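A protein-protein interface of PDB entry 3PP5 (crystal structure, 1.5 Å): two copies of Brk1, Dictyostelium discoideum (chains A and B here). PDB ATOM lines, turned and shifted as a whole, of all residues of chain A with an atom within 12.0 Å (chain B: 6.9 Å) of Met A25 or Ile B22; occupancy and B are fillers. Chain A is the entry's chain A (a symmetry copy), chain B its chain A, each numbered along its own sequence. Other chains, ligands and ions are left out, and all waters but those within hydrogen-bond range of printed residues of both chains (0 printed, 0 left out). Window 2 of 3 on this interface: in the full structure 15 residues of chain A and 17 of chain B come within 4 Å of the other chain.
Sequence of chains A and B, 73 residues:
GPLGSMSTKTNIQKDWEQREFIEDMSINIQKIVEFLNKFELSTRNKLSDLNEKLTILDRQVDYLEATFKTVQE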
ATOM      1  N   LYS A  14      14.683   4.511  -7.354  1.00  0.00           N
ATOM      2  CA  LYS A  14      15.339   4.068  -6.118  1.00  0.00           C
ATOM      3  C   LYS A  14      14.301   3.534  -5.141  1.00  0.00           C
ATOM      4  O   LYS A  14      14.511   2.491  -4.527  1.00  0.00           O
ATOM      5  CB  LYS A  14      16.130   5.212  -5.465  1.00  0.00           C
ATOM      6  CG  LYS A  14      17.387   5.601  -6.207  1.00  0.00           C
ATOM      7  CD  LYS A  14      18.041   6.814  -5.554  1.00  0.00           C
ATOM      8  CE  LYS A  14      19.214   7.289  -6.376  1.00  0.00           C
ATOM      9  NZ  LYS A  14      20.063   6.127  -6.744  1.00  0.00           N
ATOM     10  N   ASP A  15      13.171   4.215  -5.016  1.00  0.00           N
ATOM     11  CA  ASP A  15      12.132   3.757  -4.098  1.00  0.00           C
ATOM     12  C   ASP A  15      11.558   2.402  -4.550  1.00  0.00           C
ATOM     13  O   ASP A  15      11.318   1.497  -3.718  1.00  0.00           O
ATOM     14  CB  ASP A  15      11.010   4.788  -3.980  1.00  0.00           C
ATOM     15  CG  ASP A  15      10.047   4.452  -2.842  1.00  0.00           C
ATOM     16  OD1 ASP A  15      10.427   4.636  -1.667  1.00  0.00           O
ATOM     17  OD2 ASP A  15       8.925   3.974  -3.108  1.00  0.00           O
ATOM     18  N   TRP A  16      11.348   2.238  -5.852  1.00  0.00           N
ATOM     19  CA  TRP A  16      10.862   0.960  -6.385  1.00  0.00           C
ATOM     20  C   TRP A  16      11.844  -0.170  -6.050  1.00  0.00           C
ATOM     21  O   TRP A  16      11.446  -1.277  -5.646  1.00  0.00           O
ATOM     22  CB  TRP A  16      10.635   1.047  -7.901  1.00  0.00           C
ATOM     23  CG  TRP A  16      10.263  -0.287  -8.518  1.00  0.00           C
ATOM     24  CD1 TRP A  16       9.020  -0.850  -8.552  1.00  0.00           C
ATOM     25  CD2 TRP A  16      11.137  -1.222  -9.173  1.00  0.00           C
ATOM     26  NE1 TRP A  16       9.063  -2.068  -9.197  1.00  0.00           N
ATOM     27  CE2 TRP A  16      10.352  -2.321  -9.581  1.00  0.00           C
ATOM     28  CE3 TRP A  16      12.505  -1.232  -9.457  1.00  0.00           C
ATOM     29  CZ2 TRP A  16      10.894  -3.426 -10.252  1.00  0.00           C
ATOM     30  CZ3 TRP A  16      13.029  -2.332 -10.137  1.00  0.00           C
ATOM     31  CH2 TRP A  16      12.233  -3.401 -10.515  1.00  0.00           C
ATOM     32  N   GLU A  17      13.140   0.091  -6.217  1.00  0.00           N
ATOM     33  CA  GLU A  17      14.151  -0.933  -5.989  1.00  0.00           C
ATOM     34  C   GLU A  17      14.230  -1.286  -4.514  1.00  0.00           C
ATOM     35  O   GLU A  17      14.396  -2.477  -4.183  1.00  0.00           O
ATOM     36  CB  GLU A  17      15.525  -0.451  -6.482  1.00  0.00           C
ATOM     37  CG  GLU A  17      15.647  -0.440  -7.991  1.00  0.00           C
ATOM     38  CD  GLU A  17      17.034  -0.002  -8.479  1.00  0.00           C
ATOM     39  OE1 GLU A  17      17.915   0.254  -7.629  1.00  0.00           O
ATOM     40  OE2 GLU A  17      17.224   0.094  -9.713  1.00  0.00           O
ATOM     41  N   GLN A  18      14.124  -0.290  -3.637  1.00  0.00           N
ATOM     42  CA  GLN A  18      14.208  -0.537  -2.190  1.00  0.00           C
ATOM     43  C   GLN A  18      13.018  -1.377  -1.745  1.00  0.00           C
ATOM     44  O   GLN A  18      13.166  -2.331  -0.953  1.00  0.00           O
ATOM     45  CB  GLN A  18      14.276   0.782  -1.406  1.00  0.00           C
ATOM     46  CG  GLN A  18      15.600   1.499  -1.622  1.00  0.00           C
ATOM     47  CD  GLN A  18      15.681   2.815  -0.873  1.00  0.00           C
ATOM     48  OE1 GLN A  18      16.725   3.468  -0.862  1.00  0.00           O
ATOM     49  NE2 GLN A  18      14.573   3.213  -0.245  1.00  0.00           N
ATOM     50  N   ARG A  19      11.836  -1.080  -2.270  1.00  0.00           N
ATOM     51  CA  ARG A  19      10.646  -1.860  -1.925  1.00  0.00           C
ATOM     52  C   ARG A  19      10.742  -3.279  -2.481  1.00  0.00           C
ATOM     53  O   ARG A  19      10.388  -4.244  -1.793  1.00  0.00           O
ATOM     54  CB  ARG A  19       9.366  -1.168  -2.378  1.00  0.00           C
ATOM     55  CG  ARG A  19       9.124   0.104  -1.584  1.00  0.00           C
ATOM     56  CD  ARG A  19       7.864   0.775  -2.046  1.00  0.00           C
ATOM     57  NE  ARG A  19       7.563   1.925  -1.200  1.00  0.00           N
ATOM     58  CZ  ARG A  19       6.837   1.846  -0.085  1.00  0.00           C
ATOM     59  NH1 ARG A  19       6.326   0.679   0.295  1.00  0.00           N
ATOM     60  NH2 ARG A  19       6.611   2.929   0.647  1.00  0.00           N
ATOM     61  N   GLU A  20      11.218  -3.425  -3.715  1.00  0.00           N
ATOM     62  CA  GLU A  20      11.403  -4.764  -4.266  1.00  0.00           C
ATOM     63  C   GLU A  20      12.361  -5.577  -3.410  1.00  0.00           C
ATOM     64  O   GLU A  20      12.146  -6.781  -3.243  1.00  0.00           O
ATOM     65  CB  GLU A  20      11.939  -4.742  -5.708  1.00  0.00           C
ATOM     66  CG  GLU A  20      10.912  -4.389  -6.789  1.00  0.00           C
ATOM     67  CD  GLU A  20       9.752  -5.349  -6.801  1.00  0.00           C
ATOM     68  OE1 GLU A  20      10.005  -6.588  -6.806  1.00  0.00           O
ATOM     69  OE2 GLU A  20       8.603  -4.914  -6.858  1.00  0.00           O
ATOM     70  N   PHE A  21      13.414  -4.925  -2.892  1.00  0.00           N
ATOM     71  CA  PHE A  21      14.378  -5.651  -2.060  1.00  0.00           C
ATOM     72  C   PHE A  21      13.689  -6.236  -0.837  1.00  0.00           C
ATOM     73  O   PHE A  21      13.917  -7.414  -0.488  1.00  0.00           O
ATOM     74  CB  PHE A  21      15.493  -4.675  -1.667  1.00  0.00           C
ATOM     75  CG  PHE A  21      16.620  -5.290  -0.891  1.00  0.00           C
ATOM     76  CD1 PHE A  21      17.709  -5.830  -1.558  1.00  0.00           C
ATOM     77  CD2 PHE A  21      16.613  -5.250   0.490  1.00  0.00           C
ATOM     78  CE1 PHE A  21      18.793  -6.384  -0.831  1.00  0.00           C
ATOM     79  CE2 PHE A  21      17.701  -5.795   1.236  1.00  0.00           C
ATOM     80  CZ  PHE A  21      18.772  -6.357   0.552  1.00  0.00           C
ATOM     81  N   ILE A  22      12.856  -5.450  -0.175  1.00  0.00           N
ATOM     82  CA  ILE A  22      12.150  -5.898   1.022  1.00  0.00           C
ATOM     83  C   ILE A  22      11.088  -6.949   0.683  1.00  0.00           C
ATOM     84  O   ILE A  22      10.971  -7.982   1.358  1.00  0.00           O
ATOM     85  CB  ILE A  22      11.565  -4.701   1.775  1.00  0.00           C
ATOM     86  CG1 ILE A  22      12.705  -3.791   2.266  1.00  0.00           C
ATOM     87  CG2 ILE A  22      10.661  -5.200   2.901  1.00  0.00           C
ATOM     88  CD1 ILE A  22      12.234  -2.368   2.675  1.00  0.00           C
ATOM     89  N   GLU A  23      10.340  -6.741  -0.400  1.00  0.00           N
ATOM     90  CA  GLU A  23       9.361  -7.722  -0.861  1.00  0.00           C
ATOM     91  C   GLU A  23      10.035  -9.055  -1.143  1.00  0.00           C
ATOM     92  O   GLU A  23       9.506 -10.110  -0.809  1.00  0.00           O
ATOM     93  CB  GLU A  23       8.706  -7.203  -2.153  1.00  0.00           C
ATOM     94  CG  GLU A  23       7.806  -5.977  -1.934  1.00  0.00           C
ATOM     95  CD  GLU A  23       7.494  -5.278  -3.233  1.00  0.00           C
ATOM     96  OE1 GLU A  23       7.652  -5.908  -4.294  1.00  0.00           O
ATOM     97  OE2 GLU A  23       7.110  -4.088  -3.220  1.00  0.00           O
ATOM     98  N   ASP A  24      11.187  -9.025  -1.808  1.00  0.00           N
ATOM     99  CA  ASP A  24      11.911 -10.257  -2.112  1.00  0.00           C
ATOM    100  C   ASP A  24      12.380 -10.975  -0.852  1.00  0.00           C
ATOM    101  O   ASP A  24      12.381 -12.217  -0.817  1.00  0.00           O
ATOM    102  CB  ASP A  24      13.133  -9.924  -2.969  1.00  0.00           C
ATOM    103  CG  ASP A  24      12.793  -9.663  -4.414  1.00  0.00           C
ATOM    104  OD1 ASP A  24      11.635  -9.881  -4.852  1.00  0.00           O
ATOM    105  OD2 ASP A  24      13.725  -9.254  -5.146  1.00  0.00           O
ATOM    106  N   MET A  25      12.700 -10.254   0.216  1.00  0.00           N
ATOM    107  CA  MET A  25      13.008 -10.956   1.477  1.00  0.00           C
ATOM    108  C   MET A  25      11.766 -11.690   2.026  1.00  0.00           C
ATOM    109  O   MET A  25      11.864 -12.825   2.521  1.00  0.00           O
ATOM    110  CB  MET A  25      13.598  -9.969   2.497  1.00  0.00           C
ATOM    111  CG  MET A  25      15.002  -9.540   2.073  1.00  0.00           C
ATOM    112  SD  MET A  25      15.944  -8.765   3.378  1.00  0.00           S
ATOM    113  CE  MET A  25      14.858  -7.421   3.799  1.00  0.00           C
ATOM    114  N   SER A  26      10.589 -11.084   1.914  1.00  0.00           N
ATOM    115  CA  SER A  26       9.397 -11.756   2.395  1.00  0.00           C
ATOM    116  C   SER A  26       9.154 -13.027   1.610  1.00  0.00           C
ATOM    117  O   SER A  26       8.729 -14.063   2.153  1.00  0.00           O
ATOM    118  CB  SER A  26       8.197 -10.826   2.311  1.00  0.00           C
ATOM    119  OG  SER A  26       7.026 -11.527   2.621  1.00  0.00           O
ATOM    120  N   ILE A  27       9.449 -12.975   0.321  1.00  0.00           N
ATOM    121  CA  ILE A  27       9.264 -14.173  -0.515  1.00  0.00           C
ATOM    122  C   ILE A  27      10.305 -15.222  -0.161  1.00  0.00           C
ATOM    123  O   ILE A  27       9.962 -16.413  -0.065  1.00  0.00           O
ATOM    124  CB  ILE A  27       9.354 -13.771  -1.989  1.00  0.00           C
ATOM    125  CG1 ILE A  27       8.124 -12.921  -2.367  1.00  0.00           C
ATOM    126  CG2 ILE A  27       9.465 -15.064  -2.885  1.00  0.00           C
ATOM    127  CD1 ILE A  27       8.286 -12.184  -3.758  1.00  0.00           C
ATOM    128  N   ASN A  28      11.550 -14.802   0.041  1.00  0.00           N
ATOM    129  CA  ASN A  28      12.610 -15.760   0.383  1.00  0.00           C
ATOM    130  C   ASN A  28      12.376 -16.416   1.724  1.00  0.00           C
ATOM    131  O   ASN A  28      12.654 -17.626   1.872  1.00  0.00           O
ATOM    132  CB  ASN A  28      13.983 -15.094   0.316  1.00  0.00           C
ATOM    133  CG  ASN A  28      14.396 -14.794  -1.115  1.00  0.00           C
ATOM    134  OD1 ASN A  28      13.911 -15.441  -2.047  1.00  0.00           O
ATOM    135  ND2 ASN A  28      15.264 -13.807  -1.296  1.00  0.00           N
ATOM    136  N   ILE A  29      11.842 -15.695   2.705  1.00  0.00           N
ATOM    137  CA  ILE A  29      11.525 -16.321   3.985  1.00  0.00           C
ATOM    138  C   ILE A  29      10.442 -17.383   3.786  1.00  0.00           C
ATOM    139  O   ILE A  29      10.551 -18.476   4.326  1.00  0.00           O
ATOM    140  CB  ILE A  29      11.060 -15.214   4.970  1.00  0.00           C
ATOM    141  CG1 ILE A  29      12.241 -14.350   5.387  1.00  0.00           C
ATOM    142  CG2 ILE A  29      10.325 -15.827   6.202  1.00  0.00           C
ATOM    143  CD1 ILE A  29      11.821 -13.039   6.155  1.00  0.00           C
ATOM    144  N   GLN A  30       9.426 -17.113   2.974  1.00  0.00           N
ATOM    145  CA  GLN A  30       8.392 -18.114   2.692  1.00  0.00           C
ATOM    146  C   GLN A  30       8.962 -19.293   1.958  1.00  0.00           C
ATOM    147  O   GLN A  30       8.577 -20.438   2.268  1.00  0.00           O
ATOM    148  CB  GLN A  30       7.258 -17.458   1.891  1.00  0.00           C
ATOM    149  CG  GLN A  30       6.100 -18.405   1.620  1.00  0.00           C
ATOM    150  CD  GLN A  30       5.401 -18.873   2.886  1.00  0.00           C
ATOM    151  OE1 GLN A  30       5.407 -18.188   3.921  1.00  0.00           O
ATOM    152  NE2 GLN A  30       4.782 -20.049   2.808  1.00  0.00           N
ATOM    153  N   LYS A  31       9.905 -19.066   1.049  1.00  0.00           N
ATOM    154  CA  LYS A  31      10.495 -20.207   0.323  1.00  0.00           C
ATOM    155  C   LYS A  31      11.280 -21.070   1.302  1.00  0.00           C
ATOM    156  O   LYS A  31      11.310 -22.320   1.165  1.00  0.00           O
ATOM    157  CB  LYS A  31      11.402 -19.738  -0.794  1.00  0.00           C
ATOM    158  CG  LYS A  31      10.654 -19.076  -1.941  1.00  0.00           C
ATOM    159  CD  LYS A  31      11.620 -18.496  -2.960  1.00  0.00           C
ATOM    160  CE  LYS A  31      12.413 -19.598  -3.630  1.00  0.00           C
ATOM    161  NZ  LYS A  31      11.467 -20.497  -4.349  1.00  0.00           N
ATOM    162  N   ILE A  32      11.949 -20.447   2.267  1.00  0.00           N
ATOM    163  CA  ILE A  32      12.709 -21.201   3.275  1.00  0.00           C
ATOM    164  C   ILE A  32      11.758 -22.027   4.135  1.00  0.00           C
ATOM    165  O   ILE A  32      12.012 -23.232   4.387  1.00  0.00           O
ATOM    166  CB  ILE A  32      13.583 -20.254   4.147  1.00  0.00           C
ATOM    167  CG1 ILE A  32      14.737 -19.686   3.308  1.00  0.00           C
ATOM    168  CG2 ILE A  32      14.120 -21.007   5.395  1.00  0.00           C
ATOM    169  CD1 ILE A  32      15.441 -18.447   3.956  1.00  0.00           C
ATOM    170  N   VAL A  33      10.652 -21.453   4.579  1.00  0.00           N
ATOM    171  CA  VAL A  33       9.673 -22.182   5.390  1.00  0.00           C
ATOM    172  C   VAL A  33       9.118 -23.374   4.606  1.00  0.00           C
ATOM    173  O   VAL A  33       9.043 -24.509   5.140  1.00  0.00           O
ATOM    174  CB  VAL A  33       8.530 -21.232   5.816  1.00  0.00           C
ATOM    175  CG1 VAL A  33       7.358 -22.060   6.414  1.00  0.00           C
ATOM    176  CG2 VAL A  33       9.038 -20.218   6.831  1.00  0.00           C
ATOM    177  N   GLU A  34       8.796 -23.181   3.333  1.00  0.00           N
ATOM    178  CA  GLU A  34       8.261 -24.288   2.512  1.00  0.00           C
ATOM    179  C   GLU A  34       9.313 -25.388   2.366  1.00  0.00           C
ATOM    180  O   GLU A  34       8.984 -26.585   2.464  1.00  0.00           O
ATOM    181  CB  GLU A  34       7.759 -23.750   1.169  1.00  0.00           C
ATOM    182  CG  GLU A  34       6.572 -22.802   1.373  1.00  0.00           C
ATOM    183  CD  GLU A  34       5.924 -22.333   0.078  1.00  0.00           C
ATOM    184  OE1 GLU A  34       6.275 -22.862  -1.000  1.00  0.00           O
ATOM    185  OE2 GLU A  34       5.055 -21.427   0.154  1.00  0.00           O
ATOM    186  N   GLU B  17      20.431   3.295  11.440  1.00  0.00           N
ATOM    187  CA  GLU B  17      20.145   2.095  12.214  1.00  0.00           C
ATOM    188  C   GLU B  17      19.025   1.298  11.569  1.00  0.00           C
ATOM    189  O   GLU B  17      19.096   0.053  11.554  1.00  0.00           O
ATOM    190  CB  GLU B  17      19.759   2.463  13.655  1.00  0.00           C
ATOM    191  CG  GLU B  17      20.937   2.916  14.492  1.00  0.00           C
ATOM    192  CD  GLU B  17      20.555   3.240  15.942  1.00  0.00           C
ATOM    193  OE1 GLU B  17      19.369   3.068  16.303  1.00  0.00           O
ATOM    194  OE2 GLU B  17      21.447   3.676  16.705  1.00  0.00           O
ATOM    195  N   GLN B  18      18.004   1.979  11.054  1.00  0.00           N
ATOM    196  CA  GLN B  18      16.866   1.290  10.426  1.00  0.00           C
ATOM    197  C   GLN B  18      17.335   0.569   9.170  1.00  0.00           C
ATOM    198  O   GLN B  18      16.954  -0.592   8.916  1.00  0.00           O
ATOM    199  CB  GLN B  18      15.731   2.274  10.108  1.00  0.00           C
ATOM    200  CG  GLN B  18      15.057   2.786  11.372  1.00  0.00           C
ATOM    201  CD  GLN B  18      13.944   3.774  11.081  1.00  0.00           C
ATOM    202  OE1 GLN B  18      13.233   4.205  11.990  1.00  0.00           O
ATOM    203  NE2 GLN B  18      13.792   4.143   9.807  1.00  0.00           N
ATOM    204  N   ARG B  19      18.197   1.210   8.389  1.00  0.00           N
ATOM    205  CA  ARG B  19      18.726   0.576   7.181  1.00  0.00           C
ATOM    206  C   ARG B  19      19.636  -0.599   7.533  1.00  0.00           C
ATOM    207  O   ARG B  19      19.571  -1.653   6.889  1.00  0.00           O
ATOM    208  CB  ARG B  19      19.434   1.580   6.279  1.00  0.00           C
ATOM    209  CG  ARG B  19      18.447   2.569   5.684  1.00  0.00           C
ATOM    210  CD  ARG B  19      19.160   3.553   4.805  1.00  0.00           C
ATOM    211  NE  ARG B  19      18.200   4.423   4.133  1.00  0.00           N
ATOM    212  CZ  ARG B  19      17.642   4.130   2.958  1.00  0.00           C
ATOM    213  NH1 ARG B  19      17.971   3.007   2.326  1.00  0.00           N
ATOM    214  NH2 ARG B  19      16.765   4.958   2.407  1.00  0.00           N
ATOM    215  N   GLU B  20      20.484  -0.438   8.546  1.00  0.00           N
ATOM    216  CA  GLU B  20      21.322  -1.554   8.974  1.00  0.00           C
ATOM    217  C   GLU B  20      20.471  -2.741   9.397  1.00  0.00           C
ATOM    218  O   GLU B  20      20.854  -3.883   9.129  1.00  0.00           O
ATOM    219  CB  GLU B  20      22.252  -1.183  10.140  1.00  0.00           C
ATOM    220  CG  GLU B  20      23.480  -0.345   9.764  1.00  0.00           C
ATOM    221  CD  GLU B  20      24.352  -1.043   8.754  1.00  0.00           C
ATOM    222  OE1 GLU B  20      24.676  -2.245   8.978  1.00  0.00           O
ATOM    223  OE2 GLU B  20      24.767  -0.423   7.777  1.00  0.00           O
ATOM    224  N   PHE B  21      19.341  -2.468  10.069  1.00  0.00           N
ATOM    225  CA  PHE B  21      18.478  -3.567  10.510  1.00  0.00           C
ATOM    226  C   PHE B  21      17.991  -4.373   9.315  1.00  0.00           C
ATOM    227  O   PHE B  21      18.016  -5.623   9.345  1.00  0.00           O
ATOM    228  CB  PHE B  21      17.308  -2.964  11.296  1.00  0.00           C
ATOM    229  CG  PHE B  21      16.377  -3.970  11.907  1.00  0.00           C
ATOM    230  CD1 PHE B  21      16.621  -4.456  13.183  1.00  0.00           C
ATOM    231  CD2 PHE B  21      15.235  -4.355  11.233  1.00  0.00           C
ATOM    232  CE1 PHE B  21      15.728  -5.382  13.779  1.00  0.00           C
ATOM    233  CE2 PHE B  21      14.321  -5.279  11.824  1.00  0.00           C
ATOM    234  CZ  PHE B  21      14.594  -5.778  13.091  1.00  0.00           C
ATOM    235  N   ILE B  22      17.550  -3.699   8.266  1.00  0.00           N
ATOM    236  CA  ILE B  22      17.047  -4.365   7.070  1.00  0.00           C
ATOM    237  C   ILE B  22      18.174  -5.065   6.303  1.00  0.00           C
ATOM    238  O   ILE B  22      18.036  -6.220   5.873  1.00  0.00           O
ATOM    239  CB  ILE B  22      16.274  -3.376   6.193  1.00  0.00           C
ATOM    240  CG1 ILE B  22      15.036  -2.869   6.955  1.00  0.00           C
ATOM    241  CG2 ILE B  22      15.935  -4.035   4.858  1.00  0.00           C
ATOM    242  CD1 ILE B  22      14.414  -1.581   6.345  1.00  0.00           C
ATOM    243  N   GLU B  23      19.327  -4.411   6.172  1.00  0.00           N
ATOM    244  CA  GLU B  23      20.493  -5.021   5.538  1.00  0.00           C
ATOM    245  C   GLU B  23      20.886  -6.298   6.264  1.00  0.00           C
ATOM    246  O   GLU B  23      21.222  -7.298   5.638  1.00  0.00           O
ATOM    247  CB  GLU B  23      21.665  -4.028   5.589  1.00  0.00           C
ATOM    248  CG  GLU B  23      21.464  -2.793   4.696  1.00  0.00           C
ATOM    249  CD  GLU B  23      22.424  -1.687   5.051  1.00  0.00           C
ATOM    250  OE1 GLU B  23      23.444  -1.978   5.703  1.00  0.00           O
ATOM    251  OE2 GLU B  23      22.170  -0.511   4.711  1.00  0.00           O
ATOM    252  N   ASP B  24      20.899  -6.261   7.594  1.00  0.00           N
ATOM    253  CA  ASP B  24      21.253  -7.446   8.373  1.00  0.00           C
ATOM    254  C   ASP B  24      20.259  -8.584   8.174  1.00  0.00           C
ATOM    255  O   ASP B  24      20.665  -9.758   8.157  1.00  0.00           O
ATOM    256  CB  ASP B  24      21.285  -7.078   9.858  1.00  0.00           C
ATOM    257  CG  ASP B  24      22.532  -6.333  10.258  1.00  0.00           C
ATOM    258  OD1 ASP B  24      23.491  -6.206   9.458  1.00  0.00           O
ATOM    259  OD2 ASP B  24      22.567  -5.883  11.429  1.00  0.00           O
ATOM    260  N   MET B  25      18.987  -8.291   7.938  1.00  0.00           N
ATOM    261  CA  MET B  25      18.059  -9.388   7.597  1.00  0.00           C
ATOM    262  C   MET B  25      18.430 -10.032   6.244  1.00  0.00           C
ATOM    263  O   MET B  25      18.377 -11.264   6.090  1.00  0.00           O
ATOM    264  CB  MET B  25      16.610  -8.877   7.622  1.00  0.00           C
ATOM    265  CG  MET B  25      16.171  -8.584   9.055  1.00  0.00           C
ATOM    266  SD  MET B  25      14.403  -8.419   9.248  1.00  0.00           S
ATOM    267  CE  MET B  25      14.079  -7.105   8.094  1.00  0.00           C
ATOM    268  N   SER B  26      18.841  -9.230   5.268  1.00  0.00           N
ATOM    269  CA  SER B  26      19.223  -9.803   3.992  1.00  0.00           C
ATOM    270  C   SER B  26      20.422 -10.712   4.158  1.00  0.00           C
ATOM    271  O   SER B  26      20.533 -11.776   3.524  1.00  0.00           O
ATOM    272  CB  SER B  26      19.508  -8.703   2.983  1.00  0.00           C
ATOM    273  OG  SER B  26      20.030  -9.255   1.807  1.00  0.00           O
ATOM    274  N   ILE B  27      21.326 -10.318   5.040  1.00  0.00           N
ATOM    275  CA  ILE B  27      22.516 -11.152   5.281  1.00  0.00           C
ATOM    276  C   ILE B  27      22.123 -12.420   6.021  1.00  0.00           C
ATOM    277  O   ILE B  27      22.617 -13.506   5.674  1.00  0.00           O
ATOM    278  CB  ILE B  27      23.542 -10.339   6.074  1.00  0.00           C
ATOM    279  CG1 ILE B  27      24.111  -9.217   5.180  1.00  0.00           C
ATOM    280  CG2 ILE B  27      24.680 -11.293   6.603  1.00  0.00           C
ATOM    281  CD1 ILE B  27      24.919  -8.128   5.996  1.00  0.00           C
ATOM    282  N   ILE B  29      19.243 -14.003   5.979  1.00  0.00           N
ATOM    283  CA  ILE B  29      18.557 -14.928   5.083  1.00  0.00           C
ATOM    284  C   ILE B  29      19.583 -15.678   4.231  1.00  0.00           C
ATOM    285  O   ILE B  29      19.474 -16.886   4.064  1.00  0.00           O
ATOM    286  CB  ILE B  29      17.572 -14.115   4.201  1.00  0.00           C
ATOM    287  CG1 ILE B  29      16.392 -13.635   5.033  1.00  0.00           C
ATOM    288  CG2 ILE B  29      17.109 -14.942   2.961  1.00  0.00           C
ATOM    289  CD1 ILE B  29      15.493 -12.571   4.295  1.00  0.00           C
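Among the printed residues, pairs that only touch across the chains: Phe A21 with Ser B26 (3.4 Å), Met A25 with Ile B29 (3.7 Å), Met A25 with Ile B22 (3.7 Å), Ile A29 with Ile B29 (3.9 Å) and Met A25 with Met B25 (3.9999 Å).
SD of Met A25 sits at hydrogen-bond distance from N of Ser B26 (3.5 Å). OE1 of Gln A18 lies within hydrogen-bond range of NH1 of Arg B19, 3.5 Å away.
Of the 12 printed residues of chain B, 5 touch a printed residue of chain A. Printed residues of chain A that touch a printed residue of chain B: Gln A18, Phe A21, Met A25 and Ile A29. Among the printed residues, 7 pairs touch across the chains. Among the printed residues, no Asp or Glu carboxylate lies within 4 Å of a Lys or Arg side-chain nitrogen of the other chain.
Phe A21 touches Ser B26, but with the chains exchanged Ser A26 does not touch Phe B21 (11.8 Å). Met A25 touches its own counterpart, Met B25. Met A25 touches Ser B26, but with the chains exchanged Ser A26 does not touch Met B25 (8.1 Å). Ile A29 touches its own counterpart, Ile B29. Positions printed for both chains: 17, 18, 19, 20, 21, 22, 23, 24, 25, 26, 27 and 29.
Printed residues of chain B within 4 Å of Phe A21: Ser B26 (3.4 Å). Printed residues of chain B within 4 Å of Met A25: Ile B22, Met B25, Ser B26 and Ile B29. Of the printed residues of chain B, Ile A29 touches Ile B29. Printed residues of chain A within 4 Å of Arg B19: Gln A18 (3.5 Å). No residue of chain A comes within 4 Å of Glu B20. No residue of chain A comes within 4 Å of Phe B21. Of the printed residues of chain A, Ile B22 touches Met A25. No residue of chain A comes within 4 Å of Glu B23. No residue of chain A comes within 4 Å of Asp B24. Printed residues of chain A within 4 Å of Ser B26: Phe A21 (3.4 Å) and Met A25 (3.5 Å). Of the printed residues of chain A, Ile B29 touches Met A25 and Ile A29. The nearest printed residue of chain A that does not touch Met B25 is Ile A29 (6.1 Å).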
